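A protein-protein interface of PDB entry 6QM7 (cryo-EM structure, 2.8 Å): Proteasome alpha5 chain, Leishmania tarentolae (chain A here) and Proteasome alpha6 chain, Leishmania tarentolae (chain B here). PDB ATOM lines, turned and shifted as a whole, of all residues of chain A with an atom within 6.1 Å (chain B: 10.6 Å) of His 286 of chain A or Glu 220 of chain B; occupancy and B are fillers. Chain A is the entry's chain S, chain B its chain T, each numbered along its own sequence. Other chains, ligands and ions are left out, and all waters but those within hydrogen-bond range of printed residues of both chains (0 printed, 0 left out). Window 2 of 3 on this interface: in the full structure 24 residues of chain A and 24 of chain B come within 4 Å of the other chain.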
ATOM      1  N   ARG A 141      13.441 -18.394  15.205  1.00  0.00           N
ATOM      2  CA  ARG A 141      13.417 -19.867  15.053  1.00  0.00           C
ATOM      3  C   ARG A 141      13.304 -20.470  16.455  1.00  0.00           C
ATOM      4  O   ARG A 141      14.211 -20.285  17.276  1.00  0.00           O
ATOM      5  CB  ARG A 141      14.660 -20.337  14.293  1.00  0.00           C
ATOM      6  CG  ARG A 141      14.750 -21.834  14.036  1.00  0.00           C
ATOM      7  CD  ARG A 141      16.135 -22.365  14.374  1.00  0.00           C
ATOM      8  NE  ARG A 141      16.181 -22.798  15.762  1.00  0.00           N
ATOM      9  CZ  ARG A 141      15.743 -23.976  16.208  1.00  0.00           C
ATOM     10  NH1 ARG A 141      15.817 -24.252  17.502  1.00  0.00           N
ATOM     11  NH2 ARG A 141      15.230 -24.871  15.373  1.00  0.00           N
ATOM     12  N   ASP A 266      19.207 -17.912  14.185  1.00  0.00           N
ATOM     13  CA  ASP A 266      18.269 -18.457  15.191  1.00  0.00           C
ATOM     14  C   ASP A 266      17.199 -17.386  15.405  1.00  0.00           C
ATOM     15  O   ASP A 266      16.012 -17.723  15.406  1.00  0.00           O
ATOM     16  CB  ASP A 266      19.042 -18.924  16.427  1.00  0.00           C
ATOM     17  CG  ASP A 266      19.584 -20.355  16.332  1.00  0.00           C
ATOM     18  OD1 ASP A 266      18.967 -21.207  15.636  1.00  0.00           O
ATOM     19  OD2 ASP A 266      20.615 -20.627  16.980  1.00  0.00           O
ATOM     20  N   PHE A 281      17.103  -9.441  21.550  1.00  0.00           N
ATOM     21  CA  PHE A 281      17.316 -10.897  21.308  1.00  0.00           C
ATOM     22  C   PHE A 281      18.450 -11.427  22.191  1.00  0.00           C
ATOM     23  O   PHE A 281      18.289 -12.507  22.780  1.00  0.00           O
ATOM     24  CB  PHE A 281      17.691 -11.209  19.860  1.00  0.00           C
ATOM     25  CG  PHE A 281      16.598 -11.073  18.835  1.00  0.00           C
ATOM     26  CD1 PHE A 281      15.276 -11.345  19.145  1.00  0.00           C
ATOM     27  CD2 PHE A 281      16.912 -10.722  17.531  1.00  0.00           C
ATOM     28  CE1 PHE A 281      14.294 -11.232  18.176  1.00  0.00           C
ATOM     29  CE2 PHE A 281      15.925 -10.608  16.566  1.00  0.00           C
ATOM     30  CZ  PHE A 281      14.616 -10.857  16.891  1.00  0.00           C
ATOM     31  N   THR A 282      19.561 -10.692  22.256  1.00  0.00           N
ATOM     32  CA  THR A 282      20.749 -11.030  23.078  1.00  0.00           C
ATOM     33  C   THR A 282      20.314 -11.328  24.519  1.00  0.00           C
ATOM     34  O   THR A 282      20.833 -12.318  25.079  1.00  0.00           O
ATOM     35  CB  THR A 282      21.800  -9.915  23.030  1.00  0.00           C
ATOM     36  OG1 THR A 282      22.292  -9.842  21.693  1.00  0.00           O
ATOM     37  CG2 THR A 282      22.956 -10.140  23.983  1.00  0.00           C
ATOM     38  N   ARG A 284      16.973 -11.844  25.669  1.00  0.00           N
ATOM     39  CA  ARG A 284      15.667 -12.562  25.810  1.00  0.00           C
ATOM     40  C   ARG A 284      15.657 -13.921  25.089  1.00  0.00           C
ATOM     41  O   ARG A 284      15.166 -14.886  25.702  1.00  0.00           O
ATOM     42  CB  ARG A 284      14.514 -11.695  25.296  1.00  0.00           C
ATOM     43  CG  ARG A 284      14.294 -10.404  26.078  1.00  0.00           C
ATOM     44  CD  ARG A 284      13.274 -10.513  27.197  1.00  0.00           C
ATOM     45  NE  ARG A 284      11.938 -10.822  26.702  1.00  0.00           N
ATOM     46  CZ  ARG A 284      11.112  -9.961  26.101  1.00  0.00           C
ATOM     47  NH1 ARG A 284       9.925 -10.380  25.686  1.00  0.00           N
ATOM     48  NH2 ARG A 284      11.463  -8.698  25.904  1.00  0.00           N
ATOM     49  N   TYR A 285      16.127 -14.004  23.839  1.00  0.00           N
ATOM     50  CA  TYR A 285      16.045 -15.229  22.991  1.00  0.00           C
ATOM     51  C   TYR A 285      16.899 -16.341  23.608  1.00  0.00           C
ATOM     52  O   TYR A 285      18.079 -16.087  23.916  1.00  0.00           O
ATOM     53  CB  TYR A 285      16.510 -14.976  21.551  1.00  0.00           C
ATOM     54  CG  TYR A 285      16.503 -16.198  20.662  1.00  0.00           C
ATOM     55  CD1 TYR A 285      17.634 -16.988  20.510  1.00  0.00           C
ATOM     56  CD2 TYR A 285      15.360 -16.585  19.976  1.00  0.00           C
ATOM     57  CE1 TYR A 285      17.627 -18.124  19.710  1.00  0.00           C
ATOM     58  CE2 TYR A 285      15.339 -17.717  19.170  1.00  0.00           C
ATOM     59  CZ  TYR A 285      16.475 -18.496  19.037  1.00  0.00           C
ATOM     60  OH  TYR A 285      16.475 -19.618  18.256  1.00  0.00           O
ATOM     61  N   HIS A 286      16.302 -17.523  23.778  1.00  0.00           N
ATOM     62  CA  HIS A 286      16.991 -18.826  23.996  1.00  0.00           C
ATOM     63  C   HIS A 286      16.464 -19.827  22.961  1.00  0.00           C
ATOM     64  O   HIS A 286      15.470 -19.519  22.287  1.00  0.00           O
ATOM     65  CB  HIS A 286      16.858 -19.310  25.454  1.00  0.00           C
ATOM     66  CG  HIS A 286      15.467 -19.304  25.995  1.00  0.00           C
ATOM     67  ND1 HIS A 286      14.922 -18.188  26.612  1.00  0.00           N
ATOM     68  CD2 HIS A 286      14.511 -20.260  26.015  1.00  0.00           C
ATOM     69  CE1 HIS A 286      13.686 -18.454  26.983  1.00  0.00           C
ATOM     70  NE2 HIS A 286      13.410 -19.720  26.628  1.00  0.00           N
ATOM     71  N   ARG A 287      17.125 -20.977  22.832  1.00  0.00           N
ATOM     72  CA  ARG A 287      16.927 -21.928  21.707  1.00  0.00           C
ATOM     73  C   ARG A 287      15.732 -22.859  21.973  1.00  0.00           C
ATOM     74  O   ARG A 287      15.293 -23.509  21.009  1.00  0.00           O
ATOM     75  CB  ARG A 287      18.219 -22.718  21.477  1.00  0.00           C
ATOM     76  CG  ARG A 287      18.330 -23.345  20.092  1.00  0.00           C
ATOM     77  CD  ARG A 287      19.494 -22.832  19.263  1.00  0.00           C
ATOM     78  NE  ARG A 287      20.753 -23.039  19.976  1.00  0.00           N
ATOM     79  CZ  ARG A 287      21.673 -22.110  20.249  1.00  0.00           C
ATOM     80  NH1 ARG A 287      22.761 -22.454  20.921  1.00  0.00           N
ATOM     81  NH2 ARG A 287      21.538 -20.855  19.849  1.00  0.00           N
ATOM     82  N   ASN A 288      15.222 -22.924  23.213  1.00  0.00           N
ATOM     83  CA  ASN A 288      14.113 -23.832  23.626  1.00  0.00           C
ATOM     84  C   ASN A 288      12.850 -23.012  23.915  1.00  0.00           C
ATOM     85  O   ASN A 288      12.102 -23.383  24.838  1.00  0.00           O
ATOM     86  CB  ASN A 288      14.523 -24.699  24.820  1.00  0.00           C
ATOM     87  CG  ASN A 288      15.679 -25.621  24.496  1.00  0.00           C
ATOM     88  OD1 ASN A 288      16.713 -25.590  25.161  1.00  0.00           O
ATOM     89  ND2 ASN A 288      15.519 -26.437  23.466  1.00  0.00           N
ATOM     90  N   MET A 289      12.608 -21.960  23.130  1.00  0.00           N
ATOM     91  CA  MET A 289      11.381 -21.119  23.212  1.00  0.00           C
ATOM     92  C   MET A 289      10.181 -21.920  22.702  1.00  0.00           C
ATOM     93  O   MET A 289      10.359 -22.739  21.784  1.00  0.00           O
ATOM     94  CB  MET A 289      11.503 -19.846  22.366  1.00  0.00           C
ATOM     95  CG  MET A 289      12.213 -18.719  23.073  1.00  0.00           C
ATOM     96  SD  MET A 289      12.290 -17.234  22.055  1.00  0.00           S
ATOM     97  CE  MET A 289      11.790 -16.003  23.259  1.00  0.00           C
ATOM     98  N   THR A 290       9.010 -21.692  23.295  1.00  0.00           N
ATOM     99  CA  THR A 290       7.699 -22.105  22.733  1.00  0.00           C
ATOM    100  C   THR A 290       7.332 -21.106  21.636  1.00  0.00           C
ATOM    101  O   THR A 290       7.700 -19.925  21.774  1.00  0.00           O
ATOM    102  CB  THR A 290       6.615 -22.185  23.815  1.00  0.00           C
ATOM    103  OG1 THR A 290       6.642 -20.964  24.556  1.00  0.00           O
ATOM    104  CG2 THR A 290       6.805 -23.362  24.749  1.00  0.00           C
ATOM    105  N   GLU A 293       5.859 -18.071  23.093  1.00  0.00           N
ATOM    106  CA  GLU A 293       6.870 -17.115  23.643  1.00  0.00           C
ATOM    107  C   GLU A 293       7.566 -16.357  22.507  1.00  0.00           C
ATOM    108  O   GLU A 293       7.887 -15.162  22.707  1.00  0.00           O
ATOM    109  CB  GLU A 293       7.982 -17.811  24.436  1.00  0.00           C
ATOM    110  CG  GLU A 293       7.606 -18.205  25.852  1.00  0.00           C
ATOM    111  CD  GLU A 293       8.600 -19.169  26.483  1.00  0.00           C
ATOM    112  OE1 GLU A 293       9.780 -18.784  26.636  1.00  0.00           O
ATOM    113  OE2 GLU A 293       8.201 -20.314  26.787  1.00  0.00           O
ATOM    114  N   SER B 216      31.160 -16.518  15.984  1.00  0.00           N
ATOM    115  CA  SER B 216      30.955 -17.080  17.349  1.00  0.00           C
ATOM    116  C   SER B 216      29.590 -16.641  17.876  1.00  0.00           C
ATOM    117  O   SER B 216      29.338 -15.440  17.970  1.00  0.00           O
ATOM    118  CB  SER B 216      32.077 -16.688  18.295  1.00  0.00           C
ATOM    119  OG  SER B 216      32.432 -15.320  18.146  1.00  0.00           O
ATOM    120  N   PRO B 217      28.672 -17.588  18.204  1.00  0.00           N
ATOM    121  CA  PRO B 217      27.341 -17.262  18.731  1.00  0.00           C
ATOM    122  C   PRO B 217      27.287 -16.167  19.809  1.00  0.00           C
ATOM    123  O   PRO B 217      27.937 -16.312  20.831  1.00  0.00           O
ATOM    124  CB  PRO B 217      26.890 -18.601  19.333  1.00  0.00           C
ATOM    125  CG  PRO B 217      27.482 -19.616  18.391  1.00  0.00           C
ATOM    126  CD  PRO B 217      28.840 -19.042  18.037  1.00  0.00           C
ATOM    127  N   VAL B 218      26.521 -15.104  19.541  1.00  0.00           N
ATOM    128  CA  VAL B 218      26.281 -13.966  20.477  1.00  0.00           C
ATOM    129  C   VAL B 218      25.214 -14.417  21.485  1.00  0.00           C
ATOM    130  O   VAL B 218      24.051 -14.566  21.072  1.00  0.00           O
ATOM    131  CB  VAL B 218      25.866 -12.684  19.721  1.00  0.00           C
ATOM    132  CG1 VAL B 218      25.605 -11.524  20.676  1.00  0.00           C
ATOM    133  CG2 VAL B 218      26.891 -12.284  18.664  1.00  0.00           C
ATOM    134  N   ALA B 219      25.607 -14.646  22.746  1.00  0.00           N
ATOM    135  CA  ALA B 219      24.762 -15.182  23.845  1.00  0.00           C
ATOM    136  C   ALA B 219      24.243 -16.576  23.449  1.00  0.00           C
ATOM    137  O   ALA B 219      25.097 -17.446  23.183  1.00  0.00           O
ATOM    138  CB  ALA B 219      23.669 -14.192  24.192  1.00  0.00           C
ATOM    139  N   GLU B 220      22.920 -16.785  23.395  1.00  0.00           N
ATOM    140  CA  GLU B 220      22.261 -18.070  23.022  1.00  0.00           C
ATOM    141  C   GLU B 220      21.728 -17.975  21.578  1.00  0.00           C
ATOM    142  O   GLU B 220      20.776 -18.718  21.254  1.00  0.00           O
ATOM    143  CB  GLU B 220      21.170 -18.404  24.054  1.00  0.00           C
ATOM    144  CG  GLU B 220      21.432 -19.668  24.866  1.00  0.00           C
ATOM    145  CD  GLU B 220      20.968 -20.973  24.226  1.00  0.00           C
ATOM    146  OE1 GLU B 220      19.742 -21.225  24.209  1.00  0.00           O
ATOM    147  OE2 GLU B 220      21.831 -21.740  23.746  1.00  0.00           O
ATOM    148  N   LEU B 221      22.350 -17.142  20.726  1.00  0.00           N
ATOM    149  CA  LEU B 221      21.894 -16.821  19.340  1.00  0.00           C
ATOM    150  C   LEU B 221      22.993 -17.184  18.330  1.00  0.00           C
ATOM    151  O   LEU B 221      24.070 -16.545  18.375  1.00  0.00           O
ATOM    152  CB  LEU B 221      21.550 -15.329  19.268  1.00  0.00           C
ATOM    153  CG  LEU B 221      20.694 -14.904  18.076  1.00  0.00           C
ATOM    154  CD1 LEU B 221      19.906 -13.654  18.421  1.00  0.00           C
ATOM    155  CD2 LEU B 221      21.537 -14.697  16.816  1.00  0.00           C
ATOM    156  N   SER B 222      22.708 -18.145  17.438  1.00  0.00           N
ATOM    157  CA  SER B 222      23.652 -18.719  16.437  1.00  0.00           C
ATOM    158  C   SER B 222      23.448 -18.084  15.053  1.00  0.00           C
ATOM    159  O   SER B 222      22.305 -17.718  14.710  1.00  0.00           O
ATOM    160  CB  SER B 222      23.521 -20.224  16.366  1.00  0.00           C
ATOM    161  OG  SER B 222      24.743 -20.824  15.972  1.00  0.00           O
ATOM    162  N   SER B 223      24.543 -17.937  14.309  1.00  0.00           N
ATOM    163  CA  SER B 223      24.580 -17.718  12.842  1.00  0.00           C
ATOM    164  C   SER B 223      25.287 -18.917  12.212  1.00  0.00           C
ATOM    165  O   SER B 223      26.214 -19.461  12.846  1.00  0.00           O
ATOM    166  CB  SER B 223      25.282 -16.428  12.479  1.00  0.00           C
ATOM    167  OG  SER B 223      24.755 -15.333  13.210  1.00  0.00           O
ATOM    168  N   LYS B 373      31.293 -25.044  17.884  1.00  0.00           N
ATOM    169  CA  LYS B 373      30.231 -24.076  17.507  1.00  0.00           C
ATOM    170  C   LYS B 373      30.855 -22.903  16.718  1.00  0.00           C
ATOM    171  O   LYS B 373      30.073 -22.221  16.010  1.00  0.00           O
ATOM    172  CB  LYS B 373      29.405 -23.688  18.745  1.00  0.00           C
ATOM    173  CG  LYS B 373      29.714 -22.338  19.379  1.00  0.00           C
ATOM    174  CD  LYS B 373      28.956 -22.074  20.670  1.00  0.00           C
ATOM    175  CE  LYS B 373      29.515 -22.816  21.867  1.00  0.00           C
ATOM    176  NZ  LYS B 373      29.011 -22.245  23.138  1.00  0.00           N
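The guanidinium group (NH1) of Arg 287 of chain A is in salt-bridge range of the side-chain carboxylate (OE2) of Glu 220 of chain B, at 3.1 Å. O of Ser 222 of chain B sits at hydrogen-bond distance from N of Asp 266 of chain A (3.1 Å).
The backbone carbonyl oxygen (O) of Arg 284 of chain A is in hydrogen-bond range of a ring nitrogen (ND1) of His 286 of chain A, at 3.4 Å. O of Arg 141 of chain A sits at hydrogen-bond distance from OH of Tyr 285 of chain A, 2.6 Å away. The guanidinium group (NE) of Arg 141 of chain A is in salt-bridge range of the side-chain carboxylate (OD1) of Asp 266 of chain A (3.2 Å). The backbone carbonyl oxygen (O) of Asp 266 of chain A sits close to the side-chain hydroxyl (OH) of Tyr 285 of chain A (3.5 Å). OD2 of Asp 266 of chain A lies within salt-bridge range of NH2 of Arg 287 of chain A.
Among the printed residues, merely in contact across the chains: Thr 282 of chain A with Ala 219 of chain B, Tyr 285 of chain A with Glu 220 of chain B, Phe 281 of chain A with Leu 221 of chain B, His 286 of chain A with Glu 220 of chain B, Arg 287 of chain A with Ser 222 of chain B, Thr 282 of chain A with Val 218 of chain B and Arg 287 of chain A with Leu 221 of chain B.
Of the printed residues of chain B, Asp 266 of chain A touches Ser 222 (3.0 Å). Printed residues of chain B within 4 Å of Phe 281 of chain A: Leu 221. Printed residues of chain B within 4 Å of Thr 282 of chain A: Val 218 and Ala 219. Tyr 285 of chain A touches just one residue of chain B: Glu 220. Of chain B, only Glu 220 (3.7 Å) comes within 4 Å of His 286 of chain A. Of chain B, only Glu 220, Leu 221 and Ser 222 come within 4 Å of Arg 287 of chain A. Thr 290 of chain A touches none of the printed residues of chain B. Printed residues of chain A within 4 Å of Ala 219 of chain B: Thr 282 (3.5 Å). Printed residues of chain A within 4 Å of Leu 221 of chain B: Phe 281 and Arg 287. The nearest residue of chain B that does not touch His 286 of chain A is Leu 221 of chain B (6.5 Å). The nearest printed residue of chain A that does not touch Leu 221 of chain B is Asp 266 of chain A (4.4 Å).
Of the 9 printed residues of chain B, 5 touch a printed residue of chain A. Printed residues of chain B that touch a printed residue of chain A: Val 218, Ala 219, Glu 220, Leu 221 and Ser 222. Hydrophobic or aromatic side chains of chain B within 4 Å of the printed part of chain A: Val 218, Ala 219 and Leu 221. Among the printed residues, 9 pairs touch across the chains. Among the printed residues, Asp or Glu carboxylates within 4 Å of a Lys or Arg side-chain nitrogen of the other chain: Arg 287 of chain A with Glu 220 of chain B (3.1 Å).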
